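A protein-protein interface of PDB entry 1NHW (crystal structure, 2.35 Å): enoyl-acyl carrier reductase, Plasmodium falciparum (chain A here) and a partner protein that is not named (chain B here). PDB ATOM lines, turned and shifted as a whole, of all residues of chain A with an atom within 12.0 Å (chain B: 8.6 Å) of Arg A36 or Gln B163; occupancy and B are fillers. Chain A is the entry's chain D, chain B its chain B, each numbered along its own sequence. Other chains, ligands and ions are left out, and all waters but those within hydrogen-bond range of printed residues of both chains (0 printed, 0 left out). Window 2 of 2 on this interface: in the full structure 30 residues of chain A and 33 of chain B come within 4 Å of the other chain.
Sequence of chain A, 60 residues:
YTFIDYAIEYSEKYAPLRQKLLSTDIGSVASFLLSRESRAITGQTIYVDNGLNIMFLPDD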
ATOM      1  N   SER A  28     -20.036 -11.716   6.005  1.00  0.00           N
ATOM      2  CA  SER A  28     -19.100 -12.471   6.837  1.00  0.00           C
ATOM      3  C   SER A  28     -19.329 -12.229   8.332  1.00  0.00           C
ATOM      4  O   SER A  28     -19.161 -13.136   9.143  1.00  0.00           O
ATOM      5  CB  SER A  28     -17.656 -12.121   6.470  1.00  0.00           C
ATOM      6  OG  SER A  28     -17.406 -10.756   6.687  1.00  0.00           O
ATOM      7  N   VAL A  29     -19.706 -11.005   8.688  1.00  0.00           N
ATOM      8  CA  VAL A  29     -19.979 -10.677  10.079  1.00  0.00           C
ATOM      9  C   VAL A  29     -21.241 -11.429  10.502  1.00  0.00           C
ATOM     10  O   VAL A  29     -21.304 -11.968  11.604  1.00  0.00           O
ATOM     11  CB  VAL A  29     -20.184  -9.159  10.262  1.00  0.00           C
ATOM     12  CG1 VAL A  29     -20.512  -8.844  11.717  1.00  0.00           C
ATOM     13  CG2 VAL A  29     -18.930  -8.422   9.835  1.00  0.00           C
ATOM     14  N   ALA A  30     -22.238 -11.471   9.617  1.00  0.00           N
ATOM     15  CA  ALA A  30     -23.488 -12.182   9.893  1.00  0.00           C
ATOM     16  C   ALA A  30     -23.154 -13.645  10.095  1.00  0.00           C
ATOM     17  O   ALA A  30     -23.639 -14.292  11.013  1.00  0.00           O
ATOM     18  CB  ALA A  30     -24.454 -12.034   8.723  1.00  0.00           C
ATOM     19  N   SER A  31     -22.304 -14.156   9.219  1.00  0.00           N
ATOM     20  CA  SER A  31     -21.869 -15.542   9.261  1.00  0.00           C
ATOM     21  C   SER A  31     -21.249 -15.866  10.623  1.00  0.00           C
ATOM     22  O   SER A  31     -21.497 -16.922  11.199  1.00  0.00           O
ATOM     23  CB  SER A  31     -20.856 -15.769   8.136  1.00  0.00           C
ATOM     24  OG  SER A  31     -20.469 -17.122   8.053  1.00  0.00           O
ATOM     25  N   PHE A  32     -20.447 -14.944  11.140  1.00  0.00           N
ATOM     26  CA  PHE A  32     -19.808 -15.137  12.435  1.00  0.00           C
ATOM     27  C   PHE A  32     -20.834 -15.149  13.568  1.00  0.00           C
ATOM     28  O   PHE A  32     -20.763 -15.989  14.476  1.00  0.00           O
ATOM     29  CB  PHE A  32     -18.792 -14.023  12.694  1.00  0.00           C
ATOM     30  CG  PHE A  32     -18.323 -13.954  14.124  1.00  0.00           C
ATOM     31  CD1 PHE A  32     -17.548 -14.975  14.669  1.00  0.00           C
ATOM     32  CD2 PHE A  32     -18.676 -12.877  14.934  1.00  0.00           C
ATOM     33  CE1 PHE A  32     -17.131 -14.927  15.999  1.00  0.00           C
ATOM     34  CE2 PHE A  32     -18.264 -12.815  16.269  1.00  0.00           C
ATOM     35  CZ  PHE A  32     -17.490 -13.842  16.802  1.00  0.00           C
ATOM     36  N   LEU A  33     -21.780 -14.210  13.516  1.00  0.00           N
ATOM     37  CA  LEU A  33     -22.806 -14.107  14.548  1.00  0.00           C
ATOM     38  C   LEU A  33     -23.752 -15.303  14.559  1.00  0.00           C
ATOM     39  O   LEU A  33     -24.351 -15.614  15.588  1.00  0.00           O
ATOM     40  CB  LEU A  33     -23.598 -12.805  14.384  1.00  0.00           C
ATOM     41  CG  LEU A  33     -22.858 -11.529  14.815  1.00  0.00           C
ATOM     42  CD1 LEU A  33     -23.626 -10.295  14.378  1.00  0.00           C
ATOM     43  CD2 LEU A  33     -22.679 -11.536  16.324  1.00  0.00           C
ATOM     44  N   LEU A  34     -23.867 -15.984  13.421  1.00  0.00           N
ATOM     45  CA  LEU A  34     -24.738 -17.147  13.322  1.00  0.00           C
ATOM     46  C   LEU A  34     -24.047 -18.450  13.722  1.00  0.00           C
ATOM     47  O   LEU A  34     -24.715 -19.444  14.005  1.00  0.00           O
ATOM     48  CB  LEU A  34     -25.299 -17.266  11.898  1.00  0.00           C
ATOM     49  CG  LEU A  34     -26.327 -16.191  11.526  1.00  0.00           C
ATOM     50  CD1 LEU A  34     -26.649 -16.265  10.045  1.00  0.00           C
ATOM     51  CD2 LEU A  34     -27.591 -16.387  12.354  1.00  0.00           C
ATOM     52  N   SER A  35     -22.714 -18.445  13.759  1.00  0.00           N
ATOM     53  CA  SER A  35     -21.956 -19.642  14.129  1.00  0.00           C
ATOM     54  C   SER A  35     -21.718 -19.715  15.636  1.00  0.00           C
ATOM     55  O   SER A  35     -21.898 -18.730  16.351  1.00  0.00           O
ATOM     56  CB  SER A  35     -20.606 -19.671  13.413  1.00  0.00           C
ATOM     57  OG  SER A  35     -19.667 -18.848  14.081  1.00  0.00           O
ATOM     58  N   ARG A  36     -21.306 -20.888  16.107  1.00  0.00           N
ATOM     59  CA  ARG A  36     -21.057 -21.112  17.528  1.00  0.00           C
ATOM     60  C   ARG A  36     -19.864 -20.325  18.044  1.00  0.00           C
ATOM     61  O   ARG A  36     -19.606 -20.289  19.244  1.00  0.00           O
ATOM     62  CB  ARG A  36     -20.852 -22.604  17.796  1.00  0.00           C
ATOM     63  CG  ARG A  36     -22.126 -23.347  18.189  1.00  0.00           C
ATOM     64  CD  ARG A  36     -22.273 -23.419  19.709  1.00  0.00           C
ATOM     65  NE  ARG A  36     -21.209 -24.224  20.317  1.00  0.00           N
ATOM     66  CZ  ARG A  36     -21.036 -24.377  21.629  1.00  0.00           C
ATOM     67  NH1 ARG A  36     -21.857 -23.777  22.485  1.00  0.00           N
ATOM     68  NH2 ARG A  36     -20.042 -25.131  22.083  1.00  0.00           N
ATOM     69  N   GLU A  37     -19.146 -19.693  17.125  1.00  0.00           N
ATOM     70  CA  GLU A  37     -17.981 -18.894  17.472  1.00  0.00           C
ATOM     71  C   GLU A  37     -18.389 -17.732  18.373  1.00  0.00           C
ATOM     72  O   GLU A  37     -17.579 -17.207  19.138  1.00  0.00           O
ATOM     73  CB  GLU A  37     -17.342 -18.328  16.202  1.00  0.00           C
ATOM     74  CG  GLU A  37     -16.807 -19.354  15.218  1.00  0.00           C
ATOM     75  CD  GLU A  37     -15.459 -19.894  15.642  1.00  0.00           C
ATOM     76  OE1 GLU A  37     -15.413 -20.692  16.604  1.00  0.00           O
ATOM     77  OE2 GLU A  37     -14.442 -19.506  15.021  1.00  0.00           O
ATOM     78  N   SER A  38     -19.650 -17.328  18.274  1.00  0.00           N
ATOM     79  CA  SER A  38     -20.149 -16.203  19.053  1.00  0.00           C
ATOM     80  C   SER A  38     -21.162 -16.589  20.122  1.00  0.00           C
ATOM     81  O   SER A  38     -22.020 -15.786  20.475  1.00  0.00           O
ATOM     82  CB  SER A  38     -20.771 -15.172  18.108  1.00  0.00           C
ATOM     83  OG  SER A  38     -21.810 -15.749  17.346  1.00  0.00           O
ATOM     84  N   ARG A  39     -21.046 -17.808  20.642  1.00  0.00           N
ATOM     85  CA  ARG A  39     -21.966 -18.312  21.661  1.00  0.00           C
ATOM     86  C   ARG A  39     -22.198 -17.368  22.839  1.00  0.00           C
ATOM     87  O   ARG A  39     -23.236 -17.452  23.501  1.00  0.00           O
ATOM     88  CB  ARG A  39     -21.466 -19.654  22.212  1.00  0.00           C
ATOM     89  CG  ARG A  39     -20.165 -19.544  22.988  1.00  0.00           C
ATOM     90  CD  ARG A  39     -19.703 -20.875  23.574  1.00  0.00           C
ATOM     91  NE  ARG A  39     -20.646 -21.425  24.546  1.00  0.00           N
ATOM     92  CZ  ARG A  39     -20.303 -21.925  25.732  1.00  0.00           C
ATOM     93  NH1 ARG A  39     -19.030 -21.945  26.112  1.00  0.00           N
ATOM     94  NH2 ARG A  39     -21.235 -22.416  26.541  1.00  0.00           N
ATOM     95  N   ALA A  40     -21.239 -16.481  23.112  1.00  0.00           N
ATOM     96  CA  ALA A  40     -21.366 -15.561  24.241  1.00  0.00           C
ATOM     97  C   ALA A  40     -21.911 -14.173  23.913  1.00  0.00           C
ATOM     98  O   ALA A  40     -21.945 -13.305  24.787  1.00  0.00           O
ATOM     99  CB  ALA A  40     -20.027 -15.432  24.954  1.00  0.00           C
ATOM    100  N   ILE A  41     -22.346 -13.961  22.674  1.00  0.00           N
ATOM    101  CA  ILE A  41     -22.886 -12.663  22.265  1.00  0.00           C
ATOM    102  C   ILE A  41     -24.379 -12.749  21.937  1.00  0.00           C
ATOM    103  O   ILE A  41     -24.782 -13.511  21.067  1.00  0.00           O
ATOM    104  CB  ILE A  41     -22.151 -12.128  21.018  1.00  0.00           C
ATOM    105  CG1 ILE A  41     -20.644 -12.040  21.294  1.00  0.00           C
ATOM    106  CG2 ILE A  41     -22.686 -10.746  20.650  1.00  0.00           C
ATOM    107  CD1 ILE A  41     -19.819 -11.689  20.067  1.00  0.00           C
ATOM    108  N   THR A  42     -25.203 -11.971  22.627  1.00  0.00           N
ATOM    109  CA  THR A  42     -26.639 -11.990  22.366  1.00  0.00           C
ATOM    110  C   THR A  42     -27.263 -10.655  22.775  1.00  0.00           C
ATOM    111  O   THR A  42     -26.786 -10.002  23.705  1.00  0.00           O
ATOM    112  CB  THR A  42     -27.332 -13.173  23.126  1.00  0.00           C
ATOM    113  OG1 THR A  42     -28.574 -13.491  22.500  1.00  0.00           O
ATOM    114  CG2 THR A  42     -27.601 -12.814  24.582  1.00  0.00           C
ATOM    115  N   ASP B   2     -25.882 -27.605   8.833  1.00  0.00           N
ATOM    116  CA  ASP B   2     -26.384 -26.264   9.106  1.00  0.00           C
ATOM    117  C   ASP B   2     -27.407 -25.803   8.077  1.00  0.00           C
ATOM    118  O   ASP B   2     -27.146 -25.815   6.874  1.00  0.00           O
ATOM    119  CB  ASP B   2     -25.238 -25.251   9.148  1.00  0.00           C
ATOM    120  CG  ASP B   2     -24.309 -25.468  10.321  1.00  0.00           C
ATOM    121  OD1 ASP B   2     -24.807 -25.760  11.428  1.00  0.00           O
ATOM    122  OD2 ASP B   2     -23.081 -25.331  10.136  1.00  0.00           O
ATOM    123  N   ARG B  26     -19.173 -21.283   4.175  1.00  0.00           N
ATOM    124  CA  ARG B  26     -19.088 -22.191   5.319  1.00  0.00           C
ATOM    125  C   ARG B  26     -19.938 -23.448   5.132  1.00  0.00           C
ATOM    126  O   ARG B  26     -20.164 -24.204   6.080  1.00  0.00           O
ATOM    127  CB  ARG B  26     -19.517 -21.483   6.610  1.00  0.00           C
ATOM    128  CG  ARG B  26     -18.780 -20.191   6.895  1.00  0.00           C
ATOM    129  CD  ARG B  26     -18.806 -19.868   8.384  1.00  0.00           C
ATOM    130  NE  ARG B  26     -18.208 -18.565   8.682  1.00  0.00           N
ATOM    131  CZ  ARG B  26     -17.877 -18.149   9.904  1.00  0.00           C
ATOM    132  NH1 ARG B  26     -18.078 -18.936  10.956  1.00  0.00           N
ATOM    133  NH2 ARG B  26     -17.356 -16.939  10.078  1.00  0.00           N
ATOM    134  N   ILE B 113     -34.068 -26.372  11.978  1.00  0.00           N
ATOM    135  CA  ILE B 113     -32.963 -25.603  11.413  1.00  0.00           C
ATOM    136  C   ILE B 113     -32.258 -24.935  12.594  1.00  0.00           C
ATOM    137  O   ILE B 113     -32.720 -25.054  13.730  1.00  0.00           O
ATOM    138  CB  ILE B 113     -33.446 -24.535  10.396  1.00  0.00           C
ATOM    139  CG1 ILE B 113     -34.309 -23.481  11.085  1.00  0.00           C
ATOM    140  CG2 ILE B 113     -34.225 -25.208   9.272  1.00  0.00           C
ATOM    141  CD1 ILE B 113     -34.743 -22.355  10.158  1.00  0.00           C
ATOM    142  N   ASN B 114     -31.150 -24.242  12.345  1.00  0.00           N
ATOM    143  CA  ASN B 114     -30.416 -23.614  13.445  1.00  0.00           C
ATOM    144  C   ASN B 114     -29.954 -22.177  13.197  1.00  0.00           C
ATOM    145  O   ASN B 114     -29.238 -21.599  14.015  1.00  0.00           O
ATOM    146  CB  ASN B 114     -29.217 -24.495  13.821  1.00  0.00           C
ATOM    147  CG  ASN B 114     -28.222 -24.661  12.678  1.00  0.00           C
ATOM    148  OD1 ASN B 114     -28.579 -24.603  11.502  1.00  0.00           O
ATOM    149  ND2 ASN B 114     -26.965 -24.886  13.027  1.00  0.00           N
ATOM    150  N   MET B 115     -30.370 -21.600  12.077  1.00  0.00           N
ATOM    151  CA  MET B 115     -29.997 -20.235  11.733  1.00  0.00           C
ATOM    152  C   MET B 115     -31.162 -19.534  11.056  1.00  0.00           C
ATOM    153  O   MET B 115     -31.785 -20.082  10.151  1.00  0.00           O
ATOM    154  CB  MET B 115     -28.795 -20.225  10.794  1.00  0.00           C
ATOM    155  CG  MET B 115     -27.519 -20.777  11.392  1.00  0.00           C
ATOM    156  SD  MET B 115     -26.200 -20.795  10.152  1.00  0.00           S
ATOM    157  CE  MET B 115     -24.807 -21.409  11.132  1.00  0.00           C
ATOM    158  N   MET B 160     -36.396 -24.755  15.781  1.00  0.00           N
ATOM    159  CA  MET B 160     -34.970 -24.469  15.906  1.00  0.00           C
ATOM    160  C   MET B 160     -34.294 -25.271  17.019  1.00  0.00           C
ATOM    161  O   MET B 160     -34.851 -25.470  18.098  1.00  0.00           O
ATOM    162  CB  MET B 160     -34.745 -22.973  16.129  1.00  0.00           C
ATOM    163  CG  MET B 160     -35.171 -22.115  14.947  1.00  0.00           C
ATOM    164  SD  MET B 160     -34.710 -20.385  15.133  1.00  0.00           S
ATOM    165  CE  MET B 160     -33.165 -20.360  14.217  1.00  0.00           C
ATOM    166  N   LYS B 161     -33.083 -25.734  16.746  1.00  0.00           N
ATOM    167  CA  LYS B 161     -32.334 -26.510  17.721  1.00  0.00           C
ATOM    168  C   LYS B 161     -31.812 -25.583  18.809  1.00  0.00           C
ATOM    169  O   LYS B 161     -31.773 -24.368  18.633  1.00  0.00           O
ATOM    170  CB  LYS B 161     -31.156 -27.207  17.038  1.00  0.00           C
ATOM    171  CG  LYS B 161     -31.556 -28.041  15.833  1.00  0.00           C
ATOM    172  CD  LYS B 161     -30.344 -28.526  15.058  1.00  0.00           C
ATOM    173  CE  LYS B 161     -30.762 -29.170  13.741  1.00  0.00           C
ATOM    174  NZ  LYS B 161     -29.588 -29.594  12.928  1.00  0.00           N
ATOM    175  N   PRO B 162     -31.421 -26.146  19.960  1.00  0.00           N
ATOM    176  CA  PRO B 162     -30.900 -25.296  21.033  1.00  0.00           C
ATOM    177  C   PRO B 162     -29.594 -24.711  20.518  1.00  0.00           C
ATOM    178  O   PRO B 162     -28.973 -25.284  19.623  1.00  0.00           O
ATOM    179  CB  PRO B 162     -30.664 -26.280  22.179  1.00  0.00           C
ATOM    180  CG  PRO B 162     -31.651 -27.384  21.895  1.00  0.00           C
ATOM    181  CD  PRO B 162     -31.539 -27.545  20.402  1.00  0.00           C
ATOM    182  N   GLN B 163     -29.188 -23.577  21.080  1.00  0.00           N
ATOM    183  CA  GLN B 163     -27.958 -22.910  20.673  1.00  0.00           C
ATOM    184  C   GLN B 163     -28.012 -22.390  19.240  1.00  0.00           C
ATOM    185  O   GLN B 163     -26.983 -22.234  18.598  1.00  0.00           O
ATOM    186  CB  GLN B 163     -26.752 -23.846  20.831  1.00  0.00           C
ATOM    187  CG  GLN B 163     -26.472 -24.276  22.269  1.00  0.00           C
ATOM    188  CD  GLN B 163     -25.222 -25.131  22.386  1.00  0.00           C
ATOM    189  OE1 GLN B 163     -25.111 -26.184  21.755  1.00  0.00           O
ATOM    190  NE2 GLN B 163     -24.270 -24.679  23.199  1.00  0.00           N
ATOM    191  N   SER B 164     -29.219 -22.143  18.742  1.00  0.00           N
ATOM    192  CA  SER B 164     -29.405 -21.598  17.403  1.00  0.00           C
ATOM    193  C   SER B 164     -29.147 -20.090  17.467  1.00  0.00           C
ATOM    194  O   SER B 164     -29.060 -19.513  18.552  1.00  0.00           O
ATOM    195  CB  SER B 164     -30.833 -21.854  16.911  1.00  0.00           C
ATOM    196  OG  SER B 164     -31.000 -23.197  16.497  1.00  0.00           O
ATOM    197  N   SER B 165     -29.033 -19.449  16.310  1.00  0.00           N
ATOM    198  CA  SER B 165     -28.768 -18.016  16.280  1.00  0.00           C
ATOM    199  C   SER B 165     -29.649 -17.274  15.275  1.00  0.00           C
ATOM    200  O   SER B 165     -29.908 -17.760  14.170  1.00  0.00           O
ATOM    201  CB  SER B 165     -27.294 -17.775  15.957  1.00  0.00           C
ATOM    202  OG  SER B 165     -26.951 -16.420  16.148  1.00  0.00           O
ATOM    203  N   ILE B 166     -30.090 -16.086  15.674  1.00  0.00           N
ATOM    204  CA  ILE B 166     -30.954 -15.240  14.856  1.00  0.00           C
ATOM    205  C   ILE B 166     -30.377 -13.825  14.730  1.00  0.00           C
ATOM    206  O   ILE B 166     -29.871 -13.263  15.702  1.00  0.00           O
ATOM    207  CB  ILE B 166     -32.351 -15.134  15.503  1.00  0.00           C
ATOM    208  CG1 ILE B 166     -32.948 -16.535  15.661  1.00  0.00           C
ATOM    209  CG2 ILE B 166     -33.256 -14.199  14.679  1.00  0.00           C
ATOM    210  CD1 ILE B 166     -34.306 -16.551  16.339  1.00  0.00           C
ATOM    211  N   LEU B 203     -35.624 -15.605  24.641  1.00  0.00           N
ATOM    212  CA  LEU B 203     -35.095 -16.709  23.846  1.00  0.00           C
ATOM    213  C   LEU B 203     -33.889 -17.375  24.497  1.00  0.00           C
ATOM    214  O   LEU B 203     -33.675 -18.582  24.345  1.00  0.00           O
ATOM    215  CB  LEU B 203     -34.706 -16.231  22.441  1.00  0.00           C
ATOM    216  CG  LEU B 203     -35.838 -15.706  21.553  1.00  0.00           C
ATOM    217  CD1 LEU B 203     -35.282 -15.346  20.184  1.00  0.00           C
ATOM    218  CD2 LEU B 203     -36.927 -16.761  21.425  1.00  0.00           C
ATOM    219  N   GLY B 204     -33.101 -16.587  25.217  1.00  0.00           N
ATOM    220  CA  GLY B 204     -31.922 -17.123  25.865  1.00  0.00           C
ATOM    221  C   GLY B 204     -32.252 -17.926  27.101  1.00  0.00           C
ATOM    222  O   GLY B 204     -31.647 -18.959  27.358  1.00  0.00           O
ATOM    223  N   TYR B 207     -35.092 -21.021  25.509  1.00  0.00           N
ATOM    224  CA  TYR B 207     -34.647 -21.908  24.444  1.00  0.00           C
ATOM    225  C   TYR B 207     -33.141 -21.942  24.275  1.00  0.00           C
ATOM    226  O   TYR B 207     -32.625 -22.675  23.435  1.00  0.00           O
ATOM    227  CB  TYR B 207     -35.299 -21.492  23.129  1.00  0.00           C
ATOM    228  CG  TYR B 207     -36.791 -21.343  23.245  1.00  0.00           C
ATOM    229  CD1 TYR B 207     -37.634 -22.446  23.116  1.00  0.00           C
ATOM    230  CD2 TYR B 207     -37.361 -20.107  23.536  1.00  0.00           C
ATOM    231  CE1 TYR B 207     -39.014 -22.320  23.276  1.00  0.00           C
ATOM    232  CE2 TYR B 207     -38.734 -19.968  23.702  1.00  0.00           C
ATOM    233  CZ  TYR B 207     -39.554 -21.078  23.573  1.00  0.00           C
ATOM    234  OH  TYR B 207     -40.910 -20.949  23.770  1.00  0.00           O
ATOM    235  N   ASN B 208     -32.434 -21.146  25.066  1.00  0.00           N
ATOM    236  CA  ASN B 208     -30.985 -21.122  24.960  1.00  0.00           C
ATOM    237  C   ASN B 208     -30.626 -20.777  23.504  1.00  0.00           C
ATOM    238  O   ASN B 208     -29.744 -21.387  22.893  1.00  0.00           O
ATOM    239  CB  ASN B 208     -30.434 -22.496  25.369  1.00  0.00           C
ATOM    240  CG  ASN B 208     -28.930 -22.501  25.532  1.00  0.00           C
ATOM    241  OD1 ASN B 208     -28.352 -21.583  26.118  1.00  0.00           O
ATOM    242  ND2 ASN B 208     -28.284 -23.548  25.027  1.00  0.00           N
ATOM    243  N   ILE B 209     -31.342 -19.796  22.960  1.00  0.00           N
ATOM    244  CA  ILE B 209     -31.145 -19.320  21.595  1.00  0.00           C
ATOM    245  C   ILE B 209     -30.660 -17.867  21.640  1.00  0.00           C
ATOM    246  O   ILE B 209     -31.018 -17.115  22.553  1.00  0.00           O
ATOM    247  CB  ILE B 209     -32.461 -19.398  20.792  1.00  0.00           C
ATOM    248  CG1 ILE B 209     -32.807 -20.865  20.506  1.00  0.00           C
ATOM    249  CG2 ILE B 209     -32.338 -18.615  19.504  1.00  0.00           C
ATOM    250  CD1 ILE B 209     -34.086 -21.065  19.707  1.00  0.00           C
ATOM    251  N   ARG B 210     -29.853 -17.474  20.659  1.00  0.00           N
ATOM    252  CA  ARG B 210     -29.325 -16.115  20.622  1.00  0.00           C
ATOM    253  C   ARG B 210     -29.921 -15.276  19.508  1.00  0.00           C
ATOM    254  O   ARG B 210     -30.360 -15.806  18.483  1.00  0.00           O
ATOM    255  CB  ARG B 210     -27.801 -16.137  20.446  1.00  0.00           C
ATOM    256  CG  ARG B 210     -27.035 -16.837  21.561  1.00  0.00           C
ATOM    257  CD  ARG B 210     -25.533 -16.774  21.337  1.00  0.00           C
ATOM    258  NE  ARG B 210     -25.092 -17.528  20.165  1.00  0.00           N
ATOM    259  CZ  ARG B 210     -24.597 -16.984  19.055  1.00  0.00           C
ATOM    260  NH1 ARG B 210     -24.476 -15.659  18.952  1.00  0.00           N
ATOM    261  NH2 ARG B 210     -24.202 -17.767  18.051  1.00  0.00           N
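Printed residues of chain B within 4 Å of Leu A33: Ser B165 (2.8 Å) and Arg B210 (3.3 Å). Ser A35 touches just these residues of chain B: Arg B26 and Arg B210. Arg A36 touches just one residue of chain B: Gln B163 (2.7 Å). Of the printed residues of chain B, Ser A38 touches Arg B210. Printed residues of chain A within 4 Å of Arg B26: Ser A31, Phe A32 and Ser A35. Ile B113 touches none of the printed residues of chain A. No residue of chain A comes within 4 Å of Pro B162. Gln B163 touches one residue of chain A. No residue of chain A comes within 4 Å of Asn B208. No residue of chain A comes within 4 Å of Ile B209. Arg B210 touches six residues of chain A. The nearest residue of chain B that does not touch Arg A36 is Arg B210 (4.6 Å). The nearest residue of chain A that does not touch Gln B163 is Arg A39 (5.0 Å). The nearest printed residue of chain B that does not touch Leu A33 is Ile B166 (5.8 Å).
The guanidinium group of Arg B210 sits at hydrogen-bond distance from the backbone carbonyl oxygen of Leu A33, at 3.3 Å. NE of Arg B26 sits at hydrogen-bond distance from OG of Ser A31. The guanidinium group (NH2) of Arg B210 sits at hydrogen-bond distance from the backbone carbonyl oxygen (O) of Ser A35, 3.0 Å away. The side-chain hydroxyl (OG) of Ser B165 sits at hydrogen-bond distance from the backbone carbonyl oxygen (O) of Leu A33. The backbone carbonyl oxygen of Ser A38 is in hydrogen-bond range of the guanidinium group of Arg B210 (2.9 Å). The side-chain amide nitrogen of Gln B163 lies close to the guanidinium group of Arg A36. NH1 of Arg B210 is in hydrogen-bond range of O of Ile A41 (3.0 Å).
Printed residues of chain B that touch a printed residue of chain A: Arg B26, Met B115, Gln B163, Ser B165 and Arg B210. Hydrophobic or aromatic side chains of chain B that line the printed part of chain A: Met B115. Of the 15 printed residues of chain A, 10 touch a printed residue of chain B. Along chain A the printed residues that touch a printed residue of chain B span positions 31 to 42. Among the printed residues, no Asp or Glu carboxylate lies within 4 Å of a Lys or Arg side-chain nitrogen of the other chain.
O of Asn B114 sits at hydrogen-bond distance from N of Ser B165 (3.2 Å). The side-chain hydroxyl of Ser A38 lies within hydrogen-bond range of the backbone carbonyl oxygen of Phe A32 (3.1 Å). The backbone carbonyl oxygen (O) of Ser B164 is in hydrogen-bond range of the backbone NH (N) of Arg B210, at 3.0 Å. The side-chain hydroxyl of Ser A38 is in hydrogen-bond range of the backbone carbonyl oxygen of Leu A33. OG of Ser A38 lies within hydrogen-bond range of O of Ser A35, 3.1 Å away. The backbone NH (N) of Gln B163 is in hydrogen-bond range of the backbone carbonyl oxygen (O) of Asn B208, at 2.9 Å.
Phe A32 touches Arg B26. CE of Met B115 touches O of Leu A34, at 3.5 Å. O of Ser B165 touches CD2 of Leu A34, at 3.2 Å. NH1 of Arg B26 touches OG of Ser A35 (3.5 Å). Arg A39 touches Arg B210 (O to CD, 3.2 Å). Thr A42 touches Arg B210.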
